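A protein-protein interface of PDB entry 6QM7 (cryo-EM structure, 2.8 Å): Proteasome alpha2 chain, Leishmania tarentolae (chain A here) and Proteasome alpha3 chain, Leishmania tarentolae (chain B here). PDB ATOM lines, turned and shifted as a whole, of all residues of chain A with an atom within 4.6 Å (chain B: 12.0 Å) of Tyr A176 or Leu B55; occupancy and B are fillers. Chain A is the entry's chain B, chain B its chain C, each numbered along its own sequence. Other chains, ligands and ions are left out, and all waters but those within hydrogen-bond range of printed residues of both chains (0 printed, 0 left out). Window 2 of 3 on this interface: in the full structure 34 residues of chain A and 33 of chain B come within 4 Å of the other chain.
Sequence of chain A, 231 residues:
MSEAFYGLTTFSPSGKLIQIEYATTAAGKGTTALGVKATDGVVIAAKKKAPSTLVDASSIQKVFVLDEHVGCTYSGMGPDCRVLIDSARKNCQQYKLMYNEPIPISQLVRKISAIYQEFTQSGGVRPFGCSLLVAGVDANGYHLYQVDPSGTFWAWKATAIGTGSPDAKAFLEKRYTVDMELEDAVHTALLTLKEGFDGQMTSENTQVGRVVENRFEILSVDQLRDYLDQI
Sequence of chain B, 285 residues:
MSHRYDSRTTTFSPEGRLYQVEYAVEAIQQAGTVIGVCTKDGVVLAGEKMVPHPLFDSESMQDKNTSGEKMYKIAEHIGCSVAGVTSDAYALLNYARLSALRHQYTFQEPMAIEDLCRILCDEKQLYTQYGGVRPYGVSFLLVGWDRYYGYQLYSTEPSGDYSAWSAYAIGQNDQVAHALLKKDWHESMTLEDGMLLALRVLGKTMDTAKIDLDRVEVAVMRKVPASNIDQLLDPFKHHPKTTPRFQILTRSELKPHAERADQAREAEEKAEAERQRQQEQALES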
ATOM      1  N   VAL A  36      10.477  -0.583   4.830  1.00  0.00           N
ATOM      2  CA  VAL A  36      11.888  -1.036   4.758  1.00  0.00           C
ATOM      3  C   VAL A  36      12.665  -0.369   5.892  1.00  0.00           C
ATOM      4  O   VAL A  36      12.838   0.866   5.866  1.00  0.00           O
ATOM      5  CB  VAL A  36      12.501  -0.728   3.388  1.00  0.00           C
ATOM      6  CG1 VAL A  36      13.892  -1.333   3.288  1.00  0.00           C
ATOM      7  CG2 VAL A  36      11.603  -1.206   2.255  1.00  0.00           C
ATOM      8  N   LYS A  37      13.070  -1.184   6.862  1.00  0.00           N
ATOM      9  CA  LYS A  37      13.950  -0.776   7.981  1.00  0.00           C
ATOM     10  C   LYS A  37      15.372  -0.639   7.429  1.00  0.00           C
ATOM     11  O   LYS A  37      15.794  -1.492   6.641  1.00  0.00           O
ATOM     12  CB  LYS A  37      13.873  -1.779   9.135  1.00  0.00           C
ATOM     13  CG  LYS A  37      13.981  -1.161  10.519  1.00  0.00           C
ATOM     14  CD  LYS A  37      14.266  -2.166  11.603  1.00  0.00           C
ATOM     15  CE  LYS A  37      15.750  -2.395  11.815  1.00  0.00           C
ATOM     16  NZ  LYS A  37      16.040  -2.989  13.144  1.00  0.00           N
ATOM     17  N   TRP A 156       9.514  -6.649  11.352  1.00  0.00           N
ATOM     18  CA  TRP A 156      10.102  -6.944  10.030  1.00  0.00           C
ATOM     19  C   TRP A 156      11.286  -6.021   9.754  1.00  0.00           C
ATOM     20  O   TRP A 156      11.334  -4.919  10.329  1.00  0.00           O
ATOM     21  CB  TRP A 156       9.051  -6.758   8.955  1.00  0.00           C
ATOM     22  CG  TRP A 156       7.959  -7.770   8.997  1.00  0.00           C
ATOM     23  CD1 TRP A 156       6.738  -7.649   9.584  1.00  0.00           C
ATOM     24  CD2 TRP A 156       7.971  -9.045   8.352  1.00  0.00           C
ATOM     25  NE1 TRP A 156       5.992  -8.769   9.354  1.00  0.00           N
ATOM     26  CE2 TRP A 156       6.721  -9.643   8.600  1.00  0.00           C
ATOM     27  CE3 TRP A 156       8.908  -9.724   7.572  1.00  0.00           C
ATOM     28  CZ2 TRP A 156       6.389 -10.903   8.109  1.00  0.00           C
ATOM     29  CZ3 TRP A 156       8.584 -10.973   7.092  1.00  0.00           C
ATOM     30  CH2 TRP A 156       7.343 -11.554   7.358  1.00  0.00           C
ATOM     31  N   LYS A 157      12.197  -6.489   8.903  1.00  0.00           N
ATOM     32  CA  LYS A 157      13.305  -5.700   8.313  1.00  0.00           C
ATOM     33  C   LYS A 157      12.742  -4.978   7.099  1.00  0.00           C
ATOM     34  O   LYS A 157      13.051  -3.790   6.911  1.00  0.00           O
ATOM     35  CB  LYS A 157      14.473  -6.603   7.915  1.00  0.00           C
ATOM     36  CG  LYS A 157      15.496  -6.837   9.016  1.00  0.00           C
ATOM     37  CD  LYS A 157      16.122  -8.215   8.992  1.00  0.00           C
ATOM     38  CE  LYS A 157      17.381  -8.287   9.830  1.00  0.00           C
ATOM     39  NZ  LYS A 157      18.116  -9.550   9.584  1.00  0.00           N
ATOM     40  N   ALA A 158      11.954  -5.688   6.302  1.00  0.00           N
ATOM     41  CA  ALA A 158      11.104  -5.111   5.242  1.00  0.00           C
ATOM     42  C   ALA A 158       9.900  -6.014   5.048  1.00  0.00           C
ATOM     43  O   ALA A 158      10.049  -7.232   5.179  1.00  0.00           O
ATOM     44  CB  ALA A 158      11.883  -4.963   3.964  1.00  0.00           C
ATOM     45  N   LYS A 169       7.024  -8.711  -1.482  1.00  0.00           N
ATOM     46  CA  LYS A 169       7.862  -9.339  -0.421  1.00  0.00           C
ATOM     47  C   LYS A 169       9.012 -10.088  -1.092  1.00  0.00           C
ATOM     48  O   LYS A 169      10.160  -9.894  -0.656  1.00  0.00           O
ATOM     49  CB  LYS A 169       7.048 -10.275   0.482  1.00  0.00           C
ATOM     50  CG  LYS A 169       6.279  -9.567   1.589  1.00  0.00           C
ATOM     51  CD  LYS A 169       5.279 -10.442   2.321  1.00  0.00           C
ATOM     52  CE  LYS A 169       5.880 -11.221   3.475  1.00  0.00           C
ATOM     53  NZ  LYS A 169       4.971 -11.243   4.647  1.00  0.00           N
ATOM     54  N   LEU A 172      11.440  -7.555  -2.395  1.00  0.00           N
ATOM     55  CA  LEU A 172      12.175  -6.949  -1.248  1.00  0.00           C
ATOM     56  C   LEU A 172      13.229  -7.924  -0.707  1.00  0.00           C
ATOM     57  O   LEU A 172      14.275  -7.440  -0.257  1.00  0.00           O
ATOM     58  CB  LEU A 172      11.198  -6.560  -0.136  1.00  0.00           C
ATOM     59  CG  LEU A 172      10.559  -5.178  -0.266  1.00  0.00           C
ATOM     60  CD1 LEU A 172       9.357  -5.053   0.668  1.00  0.00           C
ATOM     61  CD2 LEU A 172      11.575  -4.077   0.009  1.00  0.00           C
ATOM     62  N   GLU A 173      12.969  -9.233  -0.738  1.00  0.00           N
ATOM     63  CA  GLU A 173      13.896 -10.276  -0.211  1.00  0.00           C
ATOM     64  C   GLU A 173      15.215 -10.236  -0.996  1.00  0.00           C
ATOM     65  O   GLU A 173      16.277 -10.278  -0.345  1.00  0.00           O
ATOM     66  CB  GLU A 173      13.257 -11.664  -0.274  1.00  0.00           C
ATOM     67  CG  GLU A 173      13.895 -12.662   0.679  1.00  0.00           C
ATOM     68  CD  GLU A 173      13.297 -14.060   0.639  1.00  0.00           C
ATOM     69  OE1 GLU A 173      14.050 -15.030   0.862  1.00  0.00           O
ATOM     70  OE2 GLU A 173      12.077 -14.181   0.392  1.00  0.00           O
ATOM     71  N   LYS A 174      15.149 -10.138  -2.329  1.00  0.00           N
ATOM     72  CA  LYS A 174      16.339 -10.054  -3.223  1.00  0.00           C
ATOM     73  C   LYS A 174      17.084  -8.748  -2.935  1.00  0.00           C
ATOM     74  O   LYS A 174      18.297  -8.794  -2.686  1.00  0.00           O
ATOM     75  CB  LYS A 174      15.968 -10.068  -4.712  1.00  0.00           C
ATOM     76  CG  LYS A 174      14.930 -11.090  -5.147  1.00  0.00           C
ATOM     77  CD  LYS A 174      14.748 -11.145  -6.654  1.00  0.00           C
ATOM     78  CE  LYS A 174      13.325 -11.461  -7.081  1.00  0.00           C
ATOM     79  NZ  LYS A 174      12.889 -12.804  -6.626  1.00  0.00           N
ATOM     80  N   ARG A 175      16.351  -7.639  -2.956  1.00  0.00           N
ATOM     81  CA  ARG A 175      16.868  -6.245  -2.975  1.00  0.00           C
ATOM     82  C   ARG A 175      17.429  -5.841  -1.607  1.00  0.00           C
ATOM     83  O   ARG A 175      18.403  -5.065  -1.583  1.00  0.00           O
ATOM     84  CB  ARG A 175      15.733  -5.307  -3.394  1.00  0.00           C
ATOM     85  CG  ARG A 175      15.714  -4.962  -4.876  1.00  0.00           C
ATOM     86  CD  ARG A 175      16.137  -3.517  -4.964  1.00  0.00           C
ATOM     87  NE  ARG A 175      16.805  -3.100  -6.161  1.00  0.00           N
ATOM     88  CZ  ARG A 175      17.331  -1.894  -6.371  1.00  0.00           C
ATOM     89  NH1 ARG A 175      17.263  -0.929  -5.462  1.00  0.00           N
ATOM     90  NH2 ARG A 175      17.928  -1.661  -7.525  1.00  0.00           N
ATOM     91  N   TYR A 176      16.825  -6.316  -0.514  1.00  0.00           N
ATOM     92  CA  TYR A 176      17.163  -5.901   0.871  1.00  0.00           C
ATOM     93  C   TYR A 176      18.544  -6.427   1.265  1.00  0.00           C
ATOM     94  O   TYR A 176      18.868  -7.591   0.955  1.00  0.00           O
ATOM     95  CB  TYR A 176      16.140  -6.405   1.893  1.00  0.00           C
ATOM     96  CG  TYR A 176      16.364  -5.841   3.272  1.00  0.00           C
ATOM     97  CD1 TYR A 176      15.985  -4.541   3.563  1.00  0.00           C
ATOM     98  CD2 TYR A 176      16.998  -6.572   4.266  1.00  0.00           C
ATOM     99  CE1 TYR A 176      16.205  -3.986   4.812  1.00  0.00           C
ATOM    100  CE2 TYR A 176      17.227  -6.031   5.525  1.00  0.00           C
ATOM    101  CZ  TYR A 176      16.831  -4.728   5.798  1.00  0.00           C
ATOM    102  OH  TYR A 176      17.044  -4.171   7.027  1.00  0.00           O
ATOM    103  N   THR A 177      19.317  -5.575   1.941  1.00  0.00           N
ATOM    104  CA  THR A 177      20.593  -5.899   2.635  1.00  0.00           C
ATOM    105  C   THR A 177      20.582  -5.210   4.006  1.00  0.00           C
ATOM    106  O   THR A 177      19.823  -4.239   4.170  1.00  0.00           O
ATOM    107  CB  THR A 177      21.809  -5.491   1.786  1.00  0.00           C
ATOM    108  OG1 THR A 177      21.639  -4.136   1.359  1.00  0.00           O
ATOM    109  CG2 THR A 177      22.015  -6.389   0.583  1.00  0.00           C
ATOM    110  N   VAL A 178      21.390  -5.694   4.949  1.00  0.00           N
ATOM    111  CA  VAL A 178      21.500  -5.136   6.331  1.00  0.00           C
ATOM    112  C   VAL A 178      22.202  -3.770   6.271  1.00  0.00           C
ATOM    113  O   VAL A 178      21.826  -2.884   7.063  1.00  0.00           O
ATOM    114  CB  VAL A 178      22.221  -6.125   7.270  1.00  0.00           C
ATOM    115  CG1 VAL A 178      22.520  -5.509   8.634  1.00  0.00           C
ATOM    116  CG2 VAL A 178      21.433  -7.426   7.414  1.00  0.00           C
ATOM    117  N   MET A 180      21.899  -1.528   3.982  1.00  0.00           N
ATOM    118  CA  MET A 180      20.906  -0.583   3.392  1.00  0.00           C
ATOM    119  C   MET A 180      20.689   0.627   4.311  1.00  0.00           C
ATOM    120  O   MET A 180      20.237   0.425   5.455  1.00  0.00           O
ATOM    121  CB  MET A 180      19.563  -1.285   3.151  1.00  0.00           C
ATOM    122  CG  MET A 180      18.557  -0.451   2.385  1.00  0.00           C
ATOM    123  SD  MET A 180      17.412  -1.459   1.402  1.00  0.00           S
ATOM    124  CE  MET A 180      18.473  -1.977   0.051  1.00  0.00           C
ATOM    125  N   MET B  50       8.079 -20.398  14.776  1.00  0.00           N
ATOM    126  CA  MET B  50       7.683 -20.375  13.344  1.00  0.00           C
ATOM    127  C   MET B  50       8.957 -20.270  12.501  1.00  0.00           C
ATOM    128  O   MET B  50       9.864 -19.509  12.903  1.00  0.00           O
ATOM    129  CB  MET B  50       6.751 -19.197  13.037  1.00  0.00           C
ATOM    130  CG  MET B  50       6.154 -19.252  11.634  1.00  0.00           C
ATOM    131  SD  MET B  50       4.371 -18.890  11.578  1.00  0.00           S
ATOM    132  CE  MET B  50       3.888 -19.763  10.087  1.00  0.00           C
ATOM    133  N   VAL B  51       9.032 -21.041  11.410  1.00  0.00           N
ATOM    134  CA  VAL B  51      10.180 -21.073  10.448  1.00  0.00           C
ATOM    135  C   VAL B  51      10.599 -19.632  10.143  1.00  0.00           C
ATOM    136  O   VAL B  51       9.786 -18.843   9.667  1.00  0.00           O
ATOM    137  CB  VAL B  51       9.837 -21.881   9.173  1.00  0.00           C
ATOM    138  CG1 VAL B  51       8.467 -21.527   8.591  1.00  0.00           C
ATOM    139  CG2 VAL B  51      10.929 -21.771   8.111  1.00  0.00           C
ATOM    140  N   PRO B  52      11.863 -19.230  10.420  1.00  0.00           N
ATOM    141  CA  PRO B  52      12.248 -17.821  10.337  1.00  0.00           C
ATOM    142  C   PRO B  52      12.465 -17.348   8.888  1.00  0.00           C
ATOM    143  O   PRO B  52      13.423 -17.781   8.264  1.00  0.00           O
ATOM    144  CB  PRO B  52      13.551 -17.756  11.148  1.00  0.00           C
ATOM    145  CG  PRO B  52      14.162 -19.128  10.958  1.00  0.00           C
ATOM    146  CD  PRO B  52      12.998 -20.091  10.785  1.00  0.00           C
ATOM    147  N   HIS B  53      11.561 -16.494   8.394  1.00  0.00           N
ATOM    148  CA  HIS B  53      11.703 -15.721   7.129  1.00  0.00           C
ATOM    149  C   HIS B  53      12.933 -14.822   7.263  1.00  0.00           C
ATOM    150  O   HIS B  53      13.175 -14.289   8.345  1.00  0.00           O
ATOM    151  CB  HIS B  53      10.408 -14.945   6.835  1.00  0.00           C
ATOM    152  CG  HIS B  53      10.282 -14.476   5.424  1.00  0.00           C
ATOM    153  ND1 HIS B  53      10.140 -13.141   5.097  1.00  0.00           N
ATOM    154  CD2 HIS B  53      10.272 -15.151   4.256  1.00  0.00           C
ATOM    155  CE1 HIS B  53      10.043 -13.014   3.790  1.00  0.00           C
ATOM    156  NE2 HIS B  53      10.129 -14.233   3.250  1.00  0.00           N
ATOM    157  N   PRO B  54      13.771 -14.631   6.213  1.00  0.00           N
ATOM    158  CA  PRO B  54      15.024 -13.882   6.363  1.00  0.00           C
ATOM    159  C   PRO B  54      14.837 -12.390   6.683  1.00  0.00           C
ATOM    160  O   PRO B  54      15.791 -11.769   7.116  1.00  0.00           O
ATOM    161  CB  PRO B  54      15.723 -14.028   5.000  1.00  0.00           C
ATOM    162  CG  PRO B  54      15.010 -15.181   4.326  1.00  0.00           C
ATOM    163  CD  PRO B  54      13.585 -15.118   4.837  1.00  0.00           C
ATOM    164  N   LEU B  55      13.627 -11.863   6.457  1.00  0.00           N
ATOM    165  CA  LEU B  55      13.261 -10.441   6.703  1.00  0.00           C
ATOM    166  C   LEU B  55      12.690 -10.239   8.116  1.00  0.00           C
ATOM    167  O   LEU B  55      12.530  -9.070   8.500  1.00  0.00           O
ATOM    168  CB  LEU B  55      12.264  -9.999   5.629  1.00  0.00           C
ATOM    169  CG  LEU B  55      12.846  -9.863   4.221  1.00  0.00           C
ATOM    170  CD1 LEU B  55      11.762  -9.463   3.228  1.00  0.00           C
ATOM    171  CD2 LEU B  55      13.998  -8.862   4.197  1.00  0.00           C
ATOM    172  N   PHE B  56      12.402 -11.308   8.870  1.00  0.00           N
ATOM    173  CA  PHE B  56      12.047 -11.199  10.310  1.00  0.00           C
ATOM    174  C   PHE B  56      13.154 -10.417  10.994  1.00  0.00           C
ATOM    175  O   PHE B  56      14.330 -10.729  10.765  1.00  0.00           O
ATOM    176  CB  PHE B  56      11.897 -12.549  11.018  1.00  0.00           C
ATOM    177  CG  PHE B  56      10.599 -13.294  10.807  1.00  0.00           C
ATOM    178  CD1 PHE B  56       9.465 -12.688  10.270  1.00  0.00           C
ATOM    179  CD2 PHE B  56      10.504 -14.621  11.193  1.00  0.00           C
ATOM    180  CE1 PHE B  56       8.288 -13.402  10.094  1.00  0.00           C
ATOM    181  CE2 PHE B  56       9.326 -15.335  11.017  1.00  0.00           C
ATOM    182  CZ  PHE B  56       8.221 -14.725  10.466  1.00  0.00           C
ATOM    183  N   ASP B  57      12.765  -9.420  11.779  1.00  0.00           N
ATOM    184  CA  ASP B  57      13.684  -8.580  12.582  1.00  0.00           C
ATOM    185  C   ASP B  57      13.463  -8.887  14.056  1.00  0.00           C
ATOM    186  O   ASP B  57      12.345  -9.290  14.411  1.00  0.00           O
ATOM    187  CB  ASP B  57      13.429  -7.102  12.309  1.00  0.00           C
ATOM    188  CG  ASP B  57      14.516  -6.184  12.828  1.00  0.00           C
ATOM    189  OD1 ASP B  57      15.610  -6.683  13.174  1.00  0.00           O
ATOM    190  OD2 ASP B  57      14.262  -4.968  12.871  1.00  0.00           O
ATOM    191  N   SER B  58      14.498  -8.717  14.875  1.00  0.00           N
ATOM    192  CA  SER B  58      14.370  -8.682  16.354  1.00  0.00           C
ATOM    193  C   SER B  58      13.803  -7.314  16.725  1.00  0.00           C
ATOM    194  O   SER B  58      14.224  -6.315  16.119  1.00  0.00           O
ATOM    195  CB  SER B  58      15.676  -8.955  17.080  1.00  0.00           C
ATOM    196  OG  SER B  58      16.218  -7.760  17.632  1.00  0.00           O
ATOM    197  N   GLU B  59      12.860  -7.290  17.659  1.00  0.00           N
ATOM    198  CA  GLU B  59      12.558  -6.077  18.458  1.00  0.00           C
ATOM    199  C   GLU B  59      13.753  -5.932  19.398  1.00  0.00           C
ATOM    200  O   GLU B  59      13.947  -6.847  20.225  1.00  0.00           O
ATOM    201  CB  GLU B  59      11.249  -6.182  19.252  1.00  0.00           C
ATOM    202  CG  GLU B  59      10.335  -7.342  18.870  1.00  0.00           C
ATOM    203  CD  GLU B  59       9.004  -7.346  19.597  1.00  0.00           C
ATOM    204  OE1 GLU B  59       8.555  -8.433  20.018  1.00  0.00           O
ATOM    205  OE2 GLU B  59       8.424  -6.259  19.757  1.00  0.00           O
ATOM    206  N   SER B  60      14.591  -4.914  19.219  1.00  0.00           N
ATOM    207  CA  SER B  60      15.889  -4.819  19.931  1.00  0.00           C
ATOM    208  C   SER B  60      15.630  -4.459  21.402  1.00  0.00           C
ATOM    209  O   SER B  60      16.121  -3.409  21.866  1.00  0.00           O
ATOM    210  CB  SER B  60      16.834  -3.868  19.232  1.00  0.00           C
ATOM    211  OG  SER B  60      17.292  -4.428  18.008  1.00  0.00           O
ATOM    212  N   GLU B  69       9.620 -15.411  21.215  1.00  0.00           N
ATOM    213  CA  GLU B  69       8.484 -15.823  20.354  1.00  0.00           C
ATOM    214  C   GLU B  69       7.525 -16.713  21.154  1.00  0.00           C
ATOM    215  O   GLU B  69       6.302 -16.566  20.989  1.00  0.00           O
ATOM    216  CB  GLU B  69       8.994 -16.557  19.114  1.00  0.00           C
ATOM    217  CG  GLU B  69       9.525 -15.624  18.036  1.00  0.00           C
ATOM    218  CD  GLU B  69      10.112 -16.321  16.818  1.00  0.00           C
ATOM    219  OE1 GLU B  69       9.394 -17.152  16.204  1.00  0.00           O
ATOM    220  OE2 GLU B  69      11.289 -16.032  16.487  1.00  0.00           O
ATOM    221  N   ASP B 214      17.493 -22.346  14.816  1.00  0.00           N
ATOM    222  CA  ASP B 214      16.672 -21.245  14.244  1.00  0.00           C
ATOM    223  C   ASP B 214      15.190 -21.430  14.602  1.00  0.00           C
ATOM    224  O   ASP B 214      14.497 -20.405  14.683  1.00  0.00           O
ATOM    225  CB  ASP B 214      16.853 -21.144  12.723  1.00  0.00           C
ATOM    226  CG  ASP B 214      17.929 -20.163  12.276  1.00  0.00           C
ATOM    227  OD1 ASP B 214      17.565 -19.024  11.913  1.00  0.00           O
ATOM    228  OD2 ASP B 214      19.117 -20.549  12.277  1.00  0.00           O
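The side-chain carboxylate (OD2) of Asp B57 is in salt-bridge range of the side-chain amino group (NZ) of Lys A37 (2.7 Å). N of Lys A157 is in hydrogen-bond range of O of Leu B55, 2.6 Å away. OE2 of Glu A173 lies within hydrogen-bond range of NE2 of His B53 (3.5 Å).
N of Lys A37 lies within hydrogen-bond range of O of Lys A157, 2.6 Å away. OH of Tyr A176 lies within hydrogen-bond range of O of Lys A37 (3.0 Å).
Among the printed residues, merely in contact across the chains: Trp A156 with His B53, Trp A156 with Leu B55, Trp A156 with Phe B56, Trp A156 with Asp B57, Lys A157 with Phe B56, Lys A157 with Asp B57, Ala A158 with Leu B55, Glu A173 with Pro B54 and Tyr A176 with Leu B55.
No residue of chain B comes within 4 Å of Val A36. Of chain B, only His B53 (3.3 Å), Leu B55 (3.5 Å), Phe B56 (3.4 Å) and Asp B57 (3.5 Å) come within 4 Å of Trp A156. Lys A157 touches just these residues of chain B: Leu B55 (2.6 Å), Phe B56 (3.6 Å) and Asp B57 (3.7 Å). Ala A158 touches just one residue of chain B: Leu B55. No residue of chain B comes within 4 Å of Lys A169. Leu A172 touches none of the printed residues of chain B. Of chain B, only Leu B55 comes within 4 Å of Tyr A176. No residue of chain B comes within 4 Å of Thr A177. No residue of chain B comes within 4 Å of Val A178. Printed residues of chain A within 4 Å of His B53: Trp A156 (3.3 Å) and Glu A173 (3.5 Å). Of chain A, only Trp A156 (3.5 Å), Lys A157 (2.6 Å), Ala A158 (3.4 Å) and Tyr A176 (3.8 Å) come within 4 Å of Leu B55. Of the printed residues of chain A, Asp B57 touches Lys A37 (2.7 Å), Trp A156 (3.5 Å) and Lys A157 (3.7 Å). Asp B214 touches none of the printed residues of chain A. The nearest printed residue of chain A that does not touch His B53 is Lys A169 (4.5 Å).
Of the 14 printed residues of chain A, 6 touch a printed residue of chain B. Hydrophobic or aromatic side chains of chain A within 4 Å of the printed part of chain B: Trp A156 and Tyr A176. Along chain A the printed residues that touch a printed residue of chain B span positions 37 to 176. Hydrophobic or aromatic side chains of chain B within 4 Å of the printed part of chain A: His B53, Pro B54, Leu B55 and Phe B56.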
